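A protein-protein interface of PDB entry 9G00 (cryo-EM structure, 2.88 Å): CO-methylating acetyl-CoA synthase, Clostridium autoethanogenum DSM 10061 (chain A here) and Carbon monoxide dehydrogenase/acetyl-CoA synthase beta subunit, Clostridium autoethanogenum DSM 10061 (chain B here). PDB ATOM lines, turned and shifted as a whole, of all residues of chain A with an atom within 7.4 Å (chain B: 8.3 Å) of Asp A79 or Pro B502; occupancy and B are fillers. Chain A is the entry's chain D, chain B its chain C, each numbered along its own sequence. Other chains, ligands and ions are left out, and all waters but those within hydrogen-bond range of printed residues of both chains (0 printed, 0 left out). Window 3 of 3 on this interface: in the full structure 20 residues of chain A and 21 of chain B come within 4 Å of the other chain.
Of the printed residues of chain B, Leu A78 touches Gly B503 and Thr B506.
Printed residues of chain B within 4 Å of Asp A79: Pro B502.
Of the printed residues of chain A, Asp B472 touches Met A77.
Ala B500 touches none of the printed residues of chain A.
Of chain A, only Asp A79 comes within 4 Å of Pro B502.
Of the printed residues of chain A, Gly B503 touches Leu A78 (3.7 Å).
Of the printed residues of chain A, Thr B506 touches Leu A78.
Cys B508 touches none of the printed residues of chain A.
The nearest residue of chain A that does not touch Pro B502 is Leu A78 (4.1 Å).
Gly B439 touches Phe A4 (O to CE1, 3.3 Å).
Asp B472 touches Met A77.
CA of Gly B503 touches CD2 of Leu A78, at 3.7 Å.
Leu A78 touches Thr B506.
Asp A79 touches Pro B502.
Printed residues of chain A that touch a printed residue of chain B: Phe A4, Met A77, Leu A78 and Asp A79.
Of the 19 printed residues of chain B, 5 touch a printed residue of chain A.
Hydrophobic or aromatic side chains of chain B within 4 Å of the printed part of chain A: Pro B502.
The backbone NH (N) of Gly B503 lies within hydrogen-bond range of the side-chain carboxylate (OD2) of Asp B472 (2.9 Å).
The backbone carbonyl oxygen of Asp A79 lies within hydrogen-bond range of the side-chain amide nitrogen of Asn A83.
The backbone carbonyl oxygen (O) of Pro B502 lies within hydrogen-bond range of the side-chain hydroxyl (OG1) of Thr B506 (3.1 Å).
NZ of Lys A80 lies within salt-bridge range of OD2 of Asp A79.
OD1 of Asp B472 is in hydrogen-bond range of N of Leu B504 (2.6 Å).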
ATOM      1  N   PHE A   4      13.083  32.287 -13.776  1.00  0.00           N
ATOM      2  CA  PHE A   4      13.607  31.314 -12.824  1.00  0.00           C
ATOM      3  C   PHE A   4      13.037  31.542 -11.433  1.00  0.00           C
ATOM      4  O   PHE A   4      12.652  30.589 -10.743  1.00  0.00           O
ATOM      5  CB  PHE A   4      15.135  31.377 -12.777  1.00  0.00           C
ATOM      6  CG  PHE A   4      15.824  30.682 -13.920  1.00  0.00           C
ATOM      7  CD1 PHE A   4      15.974  31.323 -15.150  1.00  0.00           C
ATOM      8  CD2 PHE A   4      16.323  29.388 -13.769  1.00  0.00           C
ATOM      9  CE1 PHE A   4      16.609  30.689 -16.225  1.00  0.00           C
ATOM     10  CE2 PHE A   4      16.963  28.737 -14.825  1.00  0.00           C
ATOM     11  CZ  PHE A   4      17.107  29.388 -16.064  1.00  0.00           C
ATOM     12  N   PHE A   8      10.683  29.004  -9.244  1.00  0.00           N
ATOM     13  CA  PHE A   8      11.072  28.586  -7.899  1.00  0.00           C
ATOM     14  C   PHE A   8      10.009  28.979  -6.876  1.00  0.00           C
ATOM     15  O   PHE A   8       9.641  28.175  -6.007  1.00  0.00           O
ATOM     16  CB  PHE A   8      12.441  29.176  -7.539  1.00  0.00           C
ATOM     17  CG  PHE A   8      13.592  28.648  -8.382  1.00  0.00           C
ATOM     18  CD1 PHE A   8      13.565  27.346  -8.904  1.00  0.00           C
ATOM     19  CD2 PHE A   8      14.701  29.452  -8.651  1.00  0.00           C
ATOM     20  CE1 PHE A   8      14.627  26.846  -9.690  1.00  0.00           C
ATOM     21  CE2 PHE A   8      15.777  28.981  -9.433  1.00  0.00           C
ATOM     22  CZ  PHE A   8      15.738  27.667  -9.958  1.00  0.00           C
ATOM     23  N   LEU A  71      13.995  18.296  -5.364  1.00  0.00           N
ATOM     24  CA  LEU A  71      13.898  18.753  -6.747  1.00  0.00           C
ATOM     25  C   LEU A  71      13.937  20.274  -6.888  1.00  0.00           C
ATOM     26  O   LEU A  71      13.959  20.777  -8.017  1.00  0.00           O
ATOM     27  CB  LEU A  71      12.617  18.214  -7.397  1.00  0.00           C
ATOM     28  CG  LEU A  71      12.620  16.710  -7.701  1.00  0.00           C
ATOM     29  CD1 LEU A  71      11.261  16.271  -8.233  1.00  0.00           C
ATOM     30  CD2 LEU A  71      13.736  16.346  -8.687  1.00  0.00           C
ATOM     31  N   VAL A  73      16.249  23.185  -6.412  1.00  0.00           N
ATOM     32  CA  VAL A  73      17.561  23.789  -6.202  1.00  0.00           C
ATOM     33  C   VAL A  73      17.538  25.154  -6.876  1.00  0.00           C
ATOM     34  O   VAL A  73      17.445  25.254  -8.106  1.00  0.00           O
ATOM     35  CB  VAL A  73      18.690  22.912  -6.757  1.00  0.00           C
ATOM     36  CG1 VAL A  73      20.056  23.557  -6.501  1.00  0.00           C
ATOM     37  CG2 VAL A  73      18.637  21.522  -6.135  1.00  0.00           C
ATOM     38  N   GLU A  75      19.090  27.597  -8.280  1.00  0.00           N
ATOM     39  CA  GLU A  75      20.213  28.082  -9.067  1.00  0.00           C
ATOM     40  C   GLU A  75      19.715  28.339 -10.478  1.00  0.00           C
ATOM     41  O   GLU A  75      19.032  27.491 -11.063  1.00  0.00           O
ATOM     42  CB  GLU A  75      21.370  27.077  -9.052  1.00  0.00           C
ATOM     43  CG  GLU A  75      21.954  26.893  -7.641  1.00  0.00           C
ATOM     44  CD  GLU A  75      22.863  25.680  -7.527  1.00  0.00           C
ATOM     45  OE1 GLU A  75      22.920  24.891  -8.484  1.00  0.00           O
ATOM     46  OE2 GLU A  75      23.517  25.515  -6.478  1.00  0.00           O
ATOM     47  N   GLU A  76      20.034  29.518 -11.020  1.00  0.00           N
ATOM     48  CA  GLU A  76      19.452  29.958 -12.291  1.00  0.00           C
ATOM     49  C   GLU A  76      20.185  29.305 -13.467  1.00  0.00           C
ATOM     50  O   GLU A  76      20.955  29.926 -14.203  1.00  0.00           O
ATOM     51  CB  GLU A  76      19.463  31.475 -12.380  1.00  0.00           C
ATOM     52  CG  GLU A  76      18.632  32.129 -11.266  1.00  0.00           C
ATOM     53  CD  GLU A  76      18.246  33.565 -11.579  1.00  0.00           C
ATOM     54  OE1 GLU A  76      18.847  34.149 -12.497  1.00  0.00           O
ATOM     55  OE2 GLU A  76      17.337  34.102 -10.914  1.00  0.00           O
ATOM     56  N   MET A  77      19.924  28.004 -13.626  1.00  0.00           N
ATOM     57  CA  MET A  77      20.351  27.234 -14.786  1.00  0.00           C
ATOM     58  C   MET A  77      19.162  26.394 -15.251  1.00  0.00           C
ATOM     59  O   MET A  77      18.285  26.002 -14.459  1.00  0.00           O
ATOM     60  CB  MET A  77      21.575  26.329 -14.477  1.00  0.00           C
ATOM     61  CG  MET A  77      22.804  27.070 -13.908  1.00  0.00           C
ATOM     62  SD  MET A  77      23.698  28.057 -15.135  1.00  0.00           S
ATOM     63  CE  MET A  77      24.725  26.836 -15.945  1.00  0.00           C
ATOM     64  N   LEU A  78      19.162  26.085 -16.549  1.00  0.00           N
ATOM     65  CA  LEU A  78      17.973  25.501 -17.162  1.00  0.00           C
ATOM     66  C   LEU A  78      17.614  24.164 -16.525  1.00  0.00           C
ATOM     67  O   LEU A  78      16.427  23.852 -16.338  1.00  0.00           O
ATOM     68  CB  LEU A  78      18.193  25.349 -18.669  1.00  0.00           C
ATOM     69  CG  LEU A  78      17.000  24.749 -19.432  1.00  0.00           C
ATOM     70  CD1 LEU A  78      15.759  25.638 -19.300  1.00  0.00           C
ATOM     71  CD2 LEU A  78      17.355  24.531 -20.897  1.00  0.00           C
ATOM     72  N   ASP A  79      18.621  23.355 -16.185  1.00  0.00           N
ATOM     73  CA  ASP A  79      18.343  22.050 -15.596  1.00  0.00           C
ATOM     74  C   ASP A  79      17.616  22.194 -14.261  1.00  0.00           C
ATOM     75  O   ASP A  79      16.667  21.455 -13.985  1.00  0.00           O
ATOM     76  CB  ASP A  79      19.639  21.245 -15.446  1.00  0.00           C
ATOM     77  CG  ASP A  79      20.689  21.966 -14.618  1.00  0.00           C
ATOM     78  OD1 ASP A  79      20.990  23.133 -14.938  1.00  0.00           O
ATOM     79  OD2 ASP A  79      21.195  21.380 -13.643  1.00  0.00           O
ATOM     80  N   LYS A  80      18.021  23.170 -13.434  1.00  0.00           N
ATOM     81  CA  LYS A  80      17.341  23.386 -12.156  1.00  0.00           C
ATOM     82  C   LYS A  80      15.909  23.850 -12.373  1.00  0.00           C
ATOM     83  O   LYS A  80      15.014  23.484 -11.613  1.00  0.00           O
ATOM     84  CB  LYS A  80      18.077  24.406 -11.280  1.00  0.00           C
ATOM     85  CG  LYS A  80      19.346  23.866 -10.620  1.00  0.00           C
ATOM     86  CD  LYS A  80      20.531  23.954 -11.580  1.00  0.00           C
ATOM     87  CE  LYS A  80      21.772  23.231 -11.030  1.00  0.00           C
ATOM     88  NZ  LYS A  80      21.556  21.749 -10.916  1.00  0.00           N
ATOM     89  N   LEU A  81      15.686  24.674 -13.395  1.00  0.00           N
ATOM     90  CA  LEU A  81      14.326  25.127 -13.692  1.00  0.00           C
ATOM     91  C   LEU A  81      13.426  23.955 -14.076  1.00  0.00           C
ATOM     92  O   LEU A  81      12.268  23.873 -13.643  1.00  0.00           O
ATOM     93  CB  LEU A  81      14.366  26.190 -14.790  1.00  0.00           C
ATOM     94  CG  LEU A  81      13.045  26.834 -15.223  1.00  0.00           C
ATOM     95  CD1 LEU A  81      13.285  28.271 -15.690  1.00  0.00           C
ATOM     96  CD2 LEU A  81      12.386  26.019 -16.334  1.00  0.00           C
ATOM     97  N   LEU A  82      13.937  23.038 -14.895  1.00  0.00           N
ATOM     98  CA  LEU A  82      13.155  21.857 -15.273  1.00  0.00           C
ATOM     99  C   LEU A  82      12.922  20.936 -14.074  1.00  0.00           C
ATOM    100  O   LEU A  82      11.820  20.393 -13.898  1.00  0.00           O
ATOM    101  CB  LEU A  82      13.839  21.107 -16.420  1.00  0.00           C
ATOM    102  CG  LEU A  82      14.079  21.954 -17.684  1.00  0.00           C
ATOM    103  CD1 LEU A  82      14.895  21.172 -18.709  1.00  0.00           C
ATOM    104  CD2 LEU A  82      12.778  22.444 -18.316  1.00  0.00           C
ATOM    105  N   ASN A  83      13.933  20.769 -13.218  1.00  0.00           N
ATOM    106  CA  ASN A  83      13.745  19.984 -12.000  1.00  0.00           C
ATOM    107  C   ASN A  83      12.716  20.632 -11.080  1.00  0.00           C
ATOM    108  O   ASN A  83      11.934  19.937 -10.429  1.00  0.00           O
ATOM    109  CB  ASN A  83      15.073  19.815 -11.262  1.00  0.00           C
ATOM    110  CG  ASN A  83      15.999  18.820 -11.933  1.00  0.00           C
ATOM    111  OD1 ASN A  83      15.546  17.807 -12.447  1.00  0.00           O
ATOM    112  ND2 ASN A  83      17.294  19.109 -11.940  1.00  0.00           N
ATOM    113  N   SER A  84      12.715  21.959 -10.994  1.00  0.00           N
ATOM    114  CA  SER A  84      11.726  22.647 -10.171  1.00  0.00           C
ATOM    115  C   SER A  84      10.317  22.496 -10.751  1.00  0.00           C
ATOM    116  O   SER A  84       9.334  22.360 -10.003  1.00  0.00           O
ATOM    117  CB  SER A  84      12.128  24.119 -10.030  1.00  0.00           C
ATOM    118  OG  SER A  84      11.195  24.833  -9.233  1.00  0.00           O
ATOM    119  N   GLY A  85      10.195  22.486 -12.081  1.00  0.00           N
ATOM    120  CA  GLY A  85       8.904  22.175 -12.672  1.00  0.00           C
ATOM    121  C   GLY A  85       8.439  20.777 -12.299  1.00  0.00           C
ATOM    122  O   GLY A  85       7.265  20.552 -11.968  1.00  0.00           O
ATOM    123  N   LEU A  86       9.369  19.821 -12.296  1.00  0.00           N
ATOM    124  CA  LEU A  86       9.017  18.473 -11.858  1.00  0.00           C
ATOM    125  C   LEU A  86       8.678  18.434 -10.371  1.00  0.00           C
ATOM    126  O   LEU A  86       7.875  17.603  -9.938  1.00  0.00           O
ATOM    127  CB  LEU A  86      10.158  17.506 -12.181  1.00  0.00           C
ATOM    128  CG  LEU A  86      10.416  17.329 -13.687  1.00  0.00           C
ATOM    129  CD1 LEU A  86      11.636  16.455 -13.920  1.00  0.00           C
ATOM    130  CD2 LEU A  86       9.191  16.741 -14.399  1.00  0.00           C
ATOM    131  N   GLY B 439      16.774  33.848 -19.362  1.00  0.00           N
ATOM    132  CA  GLY B 439      17.787  33.236 -18.527  1.00  0.00           C
ATOM    133  C   GLY B 439      18.216  31.852 -18.952  1.00  0.00           C
ATOM    134  O   GLY B 439      19.073  31.259 -18.288  1.00  0.00           O
ATOM    135  N   VAL B 440      17.652  31.320 -20.037  1.00  0.00           N
ATOM    136  CA  VAL B 440      18.127  30.052 -20.578  1.00  0.00           C
ATOM    137  C   VAL B 440      19.591  30.194 -20.968  1.00  0.00           C
ATOM    138  O   VAL B 440      20.408  29.295 -20.738  1.00  0.00           O
ATOM    139  CB  VAL B 440      17.247  29.595 -21.755  1.00  0.00           C
ATOM    140  CG1 VAL B 440      17.845  28.368 -22.450  1.00  0.00           C
ATOM    141  CG2 VAL B 440      15.823  29.276 -21.259  1.00  0.00           C
ATOM    142  N   LEU B 441      19.941  31.322 -21.579  1.00  0.00           N
ATOM    143  CA  LEU B 441      21.326  31.736 -21.755  1.00  0.00           C
ATOM    144  C   LEU B 441      21.629  32.833 -20.738  1.00  0.00           C
ATOM    145  O   LEU B 441      20.864  33.796 -20.605  1.00  0.00           O
ATOM    146  CB  LEU B 441      21.598  32.230 -23.179  1.00  0.00           C
ATOM    147  CG  LEU B 441      21.594  31.162 -24.286  1.00  0.00           C
ATOM    148  CD1 LEU B 441      22.060  31.821 -25.588  1.00  0.00           C
ATOM    149  CD2 LEU B 441      22.445  29.920 -23.966  1.00  0.00           C
ATOM    150  N   ILE B 469      31.257  28.613 -22.028  1.00  0.00           N
ATOM    151  CA  ILE B 469      30.157  27.816 -22.580  1.00  0.00           C
ATOM    152  C   ILE B 469      29.656  26.808 -21.549  1.00  0.00           C
ATOM    153  O   ILE B 469      28.478  26.447 -21.553  1.00  0.00           O
ATOM    154  CB  ILE B 469      30.527  27.128 -23.912  1.00  0.00           C
ATOM    155  CG1 ILE B 469      31.642  26.074 -23.717  1.00  0.00           C
ATOM    156  CG2 ILE B 469      30.820  28.199 -24.988  1.00  0.00           C
ATOM    157  CD1 ILE B 469      32.076  25.404 -25.018  1.00  0.00           C
ATOM    158  N   LYS B 470      30.525  26.339 -20.650  1.00  0.00           N
ATOM    159  CA  LYS B 470      30.060  25.485 -19.564  1.00  0.00           C
ATOM    160  C   LYS B 470      29.093  26.237 -18.651  1.00  0.00           C
ATOM    161  O   LYS B 470      28.180  25.627 -18.085  1.00  0.00           O
ATOM    162  CB  LYS B 470      31.263  24.940 -18.780  1.00  0.00           C
ATOM    163  CG  LYS B 470      30.904  24.159 -17.501  1.00  0.00           C
ATOM    164  CD  LYS B 470      29.917  23.004 -17.787  1.00  0.00           C
ATOM    165  CE  LYS B 470      30.568  21.886 -18.623  1.00  0.00           C
ATOM    166  NZ  LYS B 470      31.632  21.193 -17.828  1.00  0.00           N
ATOM    167  N   ASN B 471      29.264  27.559 -18.505  1.00  0.00           N
ATOM    168  CA  ASN B 471      28.381  28.391 -17.689  1.00  0.00           C
ATOM    169  C   ASN B 471      27.186  28.954 -18.475  1.00  0.00           C
ATOM    170  O   ASN B 471      26.612  29.974 -18.077  1.00  0.00           O
ATOM    171  CB  ASN B 471      29.173  29.539 -17.057  1.00  0.00           C
ATOM    172  CG  ASN B 471      30.112  29.066 -15.964  1.00  0.00           C
ATOM    173  OD1 ASN B 471      29.706  28.925 -14.821  1.00  0.00           O
ATOM    174  ND2 ASN B 471      31.371  28.801 -16.314  1.00  0.00           N
ATOM    175  N   ASP B 472      26.789  28.300 -19.570  1.00  0.00           N
ATOM    176  CA  ASP B 472      25.659  28.730 -20.401  1.00  0.00           C
ATOM    177  C   ASP B 472      25.836  30.175 -20.871  1.00  0.00           C
ATOM    178  O   ASP B 472      24.887  30.954 -20.926  1.00  0.00           O
ATOM    179  CB  ASP B 472      24.315  28.558 -19.684  1.00  0.00           C
ATOM    180  CG  ASP B 472      23.816  27.119 -19.714  1.00  0.00           C
ATOM    181  OD1 ASP B 472      24.235  26.384 -20.628  1.00  0.00           O
ATOM    182  OD2 ASP B 472      23.020  26.720 -18.841  1.00  0.00           O
ATOM    183  N   ALA B 496      28.629  21.165 -28.721  1.00  0.00           N
ATOM    184  CA  ALA B 496      27.540  21.561 -27.833  1.00  0.00           C
ATOM    185  C   ALA B 496      27.283  20.529 -26.741  1.00  0.00           C
ATOM    186  O   ALA B 496      27.316  20.862 -25.544  1.00  0.00           O
ATOM    187  CB  ALA B 496      26.266  21.799 -28.654  1.00  0.00           C
ATOM    188  N   TYR B 499      30.808  20.178 -24.288  1.00  0.00           N
ATOM    189  CA  TYR B 499      31.363  21.219 -23.427  1.00  0.00           C
ATOM    190  C   TYR B 499      30.315  22.154 -22.843  1.00  0.00           C
ATOM    191  O   TYR B 499      30.516  22.695 -21.753  1.00  0.00           O
ATOM    192  CB  TYR B 499      32.390  22.057 -24.196  1.00  0.00           C
ATOM    193  CG  TYR B 499      33.510  21.256 -24.785  1.00  0.00           C
ATOM    194  CD1 TYR B 499      34.444  20.618 -23.965  1.00  0.00           C
ATOM    195  CD2 TYR B 499      33.647  21.133 -26.164  1.00  0.00           C
ATOM    196  CE1 TYR B 499      35.493  19.870 -24.513  1.00  0.00           C
ATOM    197  CE2 TYR B 499      34.685  20.398 -26.728  1.00  0.00           C
ATOM    198  CZ  TYR B 499      35.601  19.770 -25.896  1.00  0.00           C
ATOM    199  OH  TYR B 499      36.622  19.043 -26.475  1.00  0.00           O
ATOM    200  N   ALA B 500      29.205  22.363 -23.545  1.00  0.00           N
ATOM    201  CA  ALA B 500      28.258  23.382 -23.123  1.00  0.00           C
ATOM    202  C   ALA B 500      27.434  22.928 -21.918  1.00  0.00           C
ATOM    203  O   ALA B 500      27.279  21.735 -21.654  1.00  0.00           O
ATOM    204  CB  ALA B 500      27.335  23.755 -24.282  1.00  0.00           C
ATOM    205  N   GLY B 501      26.940  23.912 -21.156  1.00  0.00           N
ATOM    206  CA  GLY B 501      26.020  23.647 -20.075  1.00  0.00           C
ATOM    207  C   GLY B 501      24.630  23.343 -20.605  1.00  0.00           C
ATOM    208  O   GLY B 501      24.380  23.348 -21.806  1.00  0.00           O
ATOM    209  N   PRO B 502      23.692  23.075 -19.694  1.00  0.00           N
ATOM    210  CA  PRO B 502      22.350  22.625 -20.148  1.00  0.00           C
ATOM    211  C   PRO B 502      21.603  23.632 -21.011  1.00  0.00           C
ATOM    212  O   PRO B 502      21.077  23.258 -22.067  1.00  0.00           O
ATOM    213  CB  PRO B 502      21.617  22.321 -18.826  1.00  0.00           C
ATOM    214  CG  PRO B 502      22.350  23.171 -17.771  1.00  0.00           C
ATOM    215  CD  PRO B 502      23.791  23.185 -18.225  1.00  0.00           C
ATOM    216  N   GLY B 503      21.548  24.899 -20.602  1.00  0.00           N
ATOM    217  CA  GLY B 503      20.813  25.884 -21.375  1.00  0.00           C
ATOM    218  C   GLY B 503      21.422  26.117 -22.745  1.00  0.00           C
ATOM    219  O   GLY B 503      20.713  26.182 -23.754  1.00  0.00           O
ATOM    220  N   LEU B 504      22.746  26.249 -22.801  1.00  0.00           N
ATOM    221  CA  LEU B 504      23.410  26.455 -24.083  1.00  0.00           C
ATOM    222  C   LEU B 504      23.317  25.213 -24.965  1.00  0.00           C
ATOM    223  O   LEU B 504      23.161  25.332 -26.181  1.00  0.00           O
ATOM    224  CB  LEU B 504      24.869  26.870 -23.869  1.00  0.00           C
ATOM    225  CG  LEU B 504      25.677  27.222 -25.137  1.00  0.00           C
ATOM    226  CD1 LEU B 504      24.948  28.214 -26.058  1.00  0.00           C
ATOM    227  CD2 LEU B 504      27.065  27.765 -24.738  1.00  0.00           C
ATOM    228  N   ALA B 505      23.390  24.012 -24.382  1.00  0.00           N
ATOM    229  CA  ALA B 505      23.224  22.790 -25.169  1.00  0.00           C
ATOM    230  C   ALA B 505      21.825  22.721 -25.772  1.00  0.00           C
ATOM    231  O   ALA B 505      21.662  22.357 -26.943  1.00  0.00           O
ATOM    232  CB  ALA B 505      23.503  21.548 -24.313  1.00  0.00           C
ATOM    233  N   THR B 506      20.804  23.074 -24.990  1.00  0.00           N
ATOM    234  CA  THR B 506      19.449  23.118 -25.527  1.00  0.00           C
ATOM    235  C   THR B 506      19.337  24.141 -26.651  1.00  0.00           C
ATOM    236  O   THR B 506      18.763  23.849 -27.706  1.00  0.00           O
ATOM    237  CB  THR B 506      18.454  23.453 -24.414  1.00  0.00           C
ATOM    238  OG1 THR B 506      18.439  22.407 -23.436  1.00  0.00           O
ATOM    239  CG2 THR B 506      17.045  23.636 -24.976  1.00  0.00           C
ATOM    240  N   VAL B 507      19.911  25.330 -26.464  1.00  0.00           N
ATOM    241  CA  VAL B 507      19.844  26.357 -27.505  1.00  0.00           C
ATOM    242  C   VAL B 507      20.541  25.879 -28.773  1.00  0.00           C
ATOM    243  O   VAL B 507      20.028  26.051 -29.886  1.00  0.00           O
ATOM    244  CB  VAL B 507      20.434  27.682 -26.989  1.00  0.00           C
ATOM    245  CG1 VAL B 507      20.597  28.695 -28.122  1.00  0.00           C
ATOM    246  CG2 VAL B 507      19.545  28.265 -25.891  1.00  0.00           C
ATOM    247  N   CYS B 508      21.715  25.266 -28.628  1.00  0.00           N
ATOM    248  CA  CYS B 508      22.446  24.783 -29.792  1.00  0.00           C
ATOM    249  C   CYS B 508      21.667  23.698 -30.513  1.00  0.00           C
ATOM    250  O   CYS B 508      21.654  23.658 -31.741  1.00  0.00           O
ATOM    251  CB  CYS B 508      23.815  24.240 -29.378  1.00  0.00           C
ATOM    252  SG  CYS B 508      24.988  25.509 -28.896  1.00  0.00           S
ATOM    253  N   LYS B 509      21.033  22.798 -29.772  1.00  0.00           N
ATOM    254  CA  LYS B 509      20.225  21.770 -30.418  1.00  0.00           C
ATOM    255  C   LYS B 509      19.032  22.372 -31.153  1.00  0.00           C
ATOM    256  O   LYS B 509      18.750  22.007 -32.299  1.00  0.00           O
ATOM    257  CB  LYS B 509      19.781  20.746 -29.376  1.00  0.00           C
ATOM    258  CG  LYS B 509      19.061  19.546 -29.976  1.00  0.00           C
ATOM    259  CD  LYS B 509      18.803  18.468 -28.915  1.00  0.00           C
ATOM    260  CE  LYS B 509      17.955  19.004 -27.743  1.00  0.00           C
ATOM    261  NZ  LYS B 509      16.620  19.536 -28.195  1.00  0.00           N
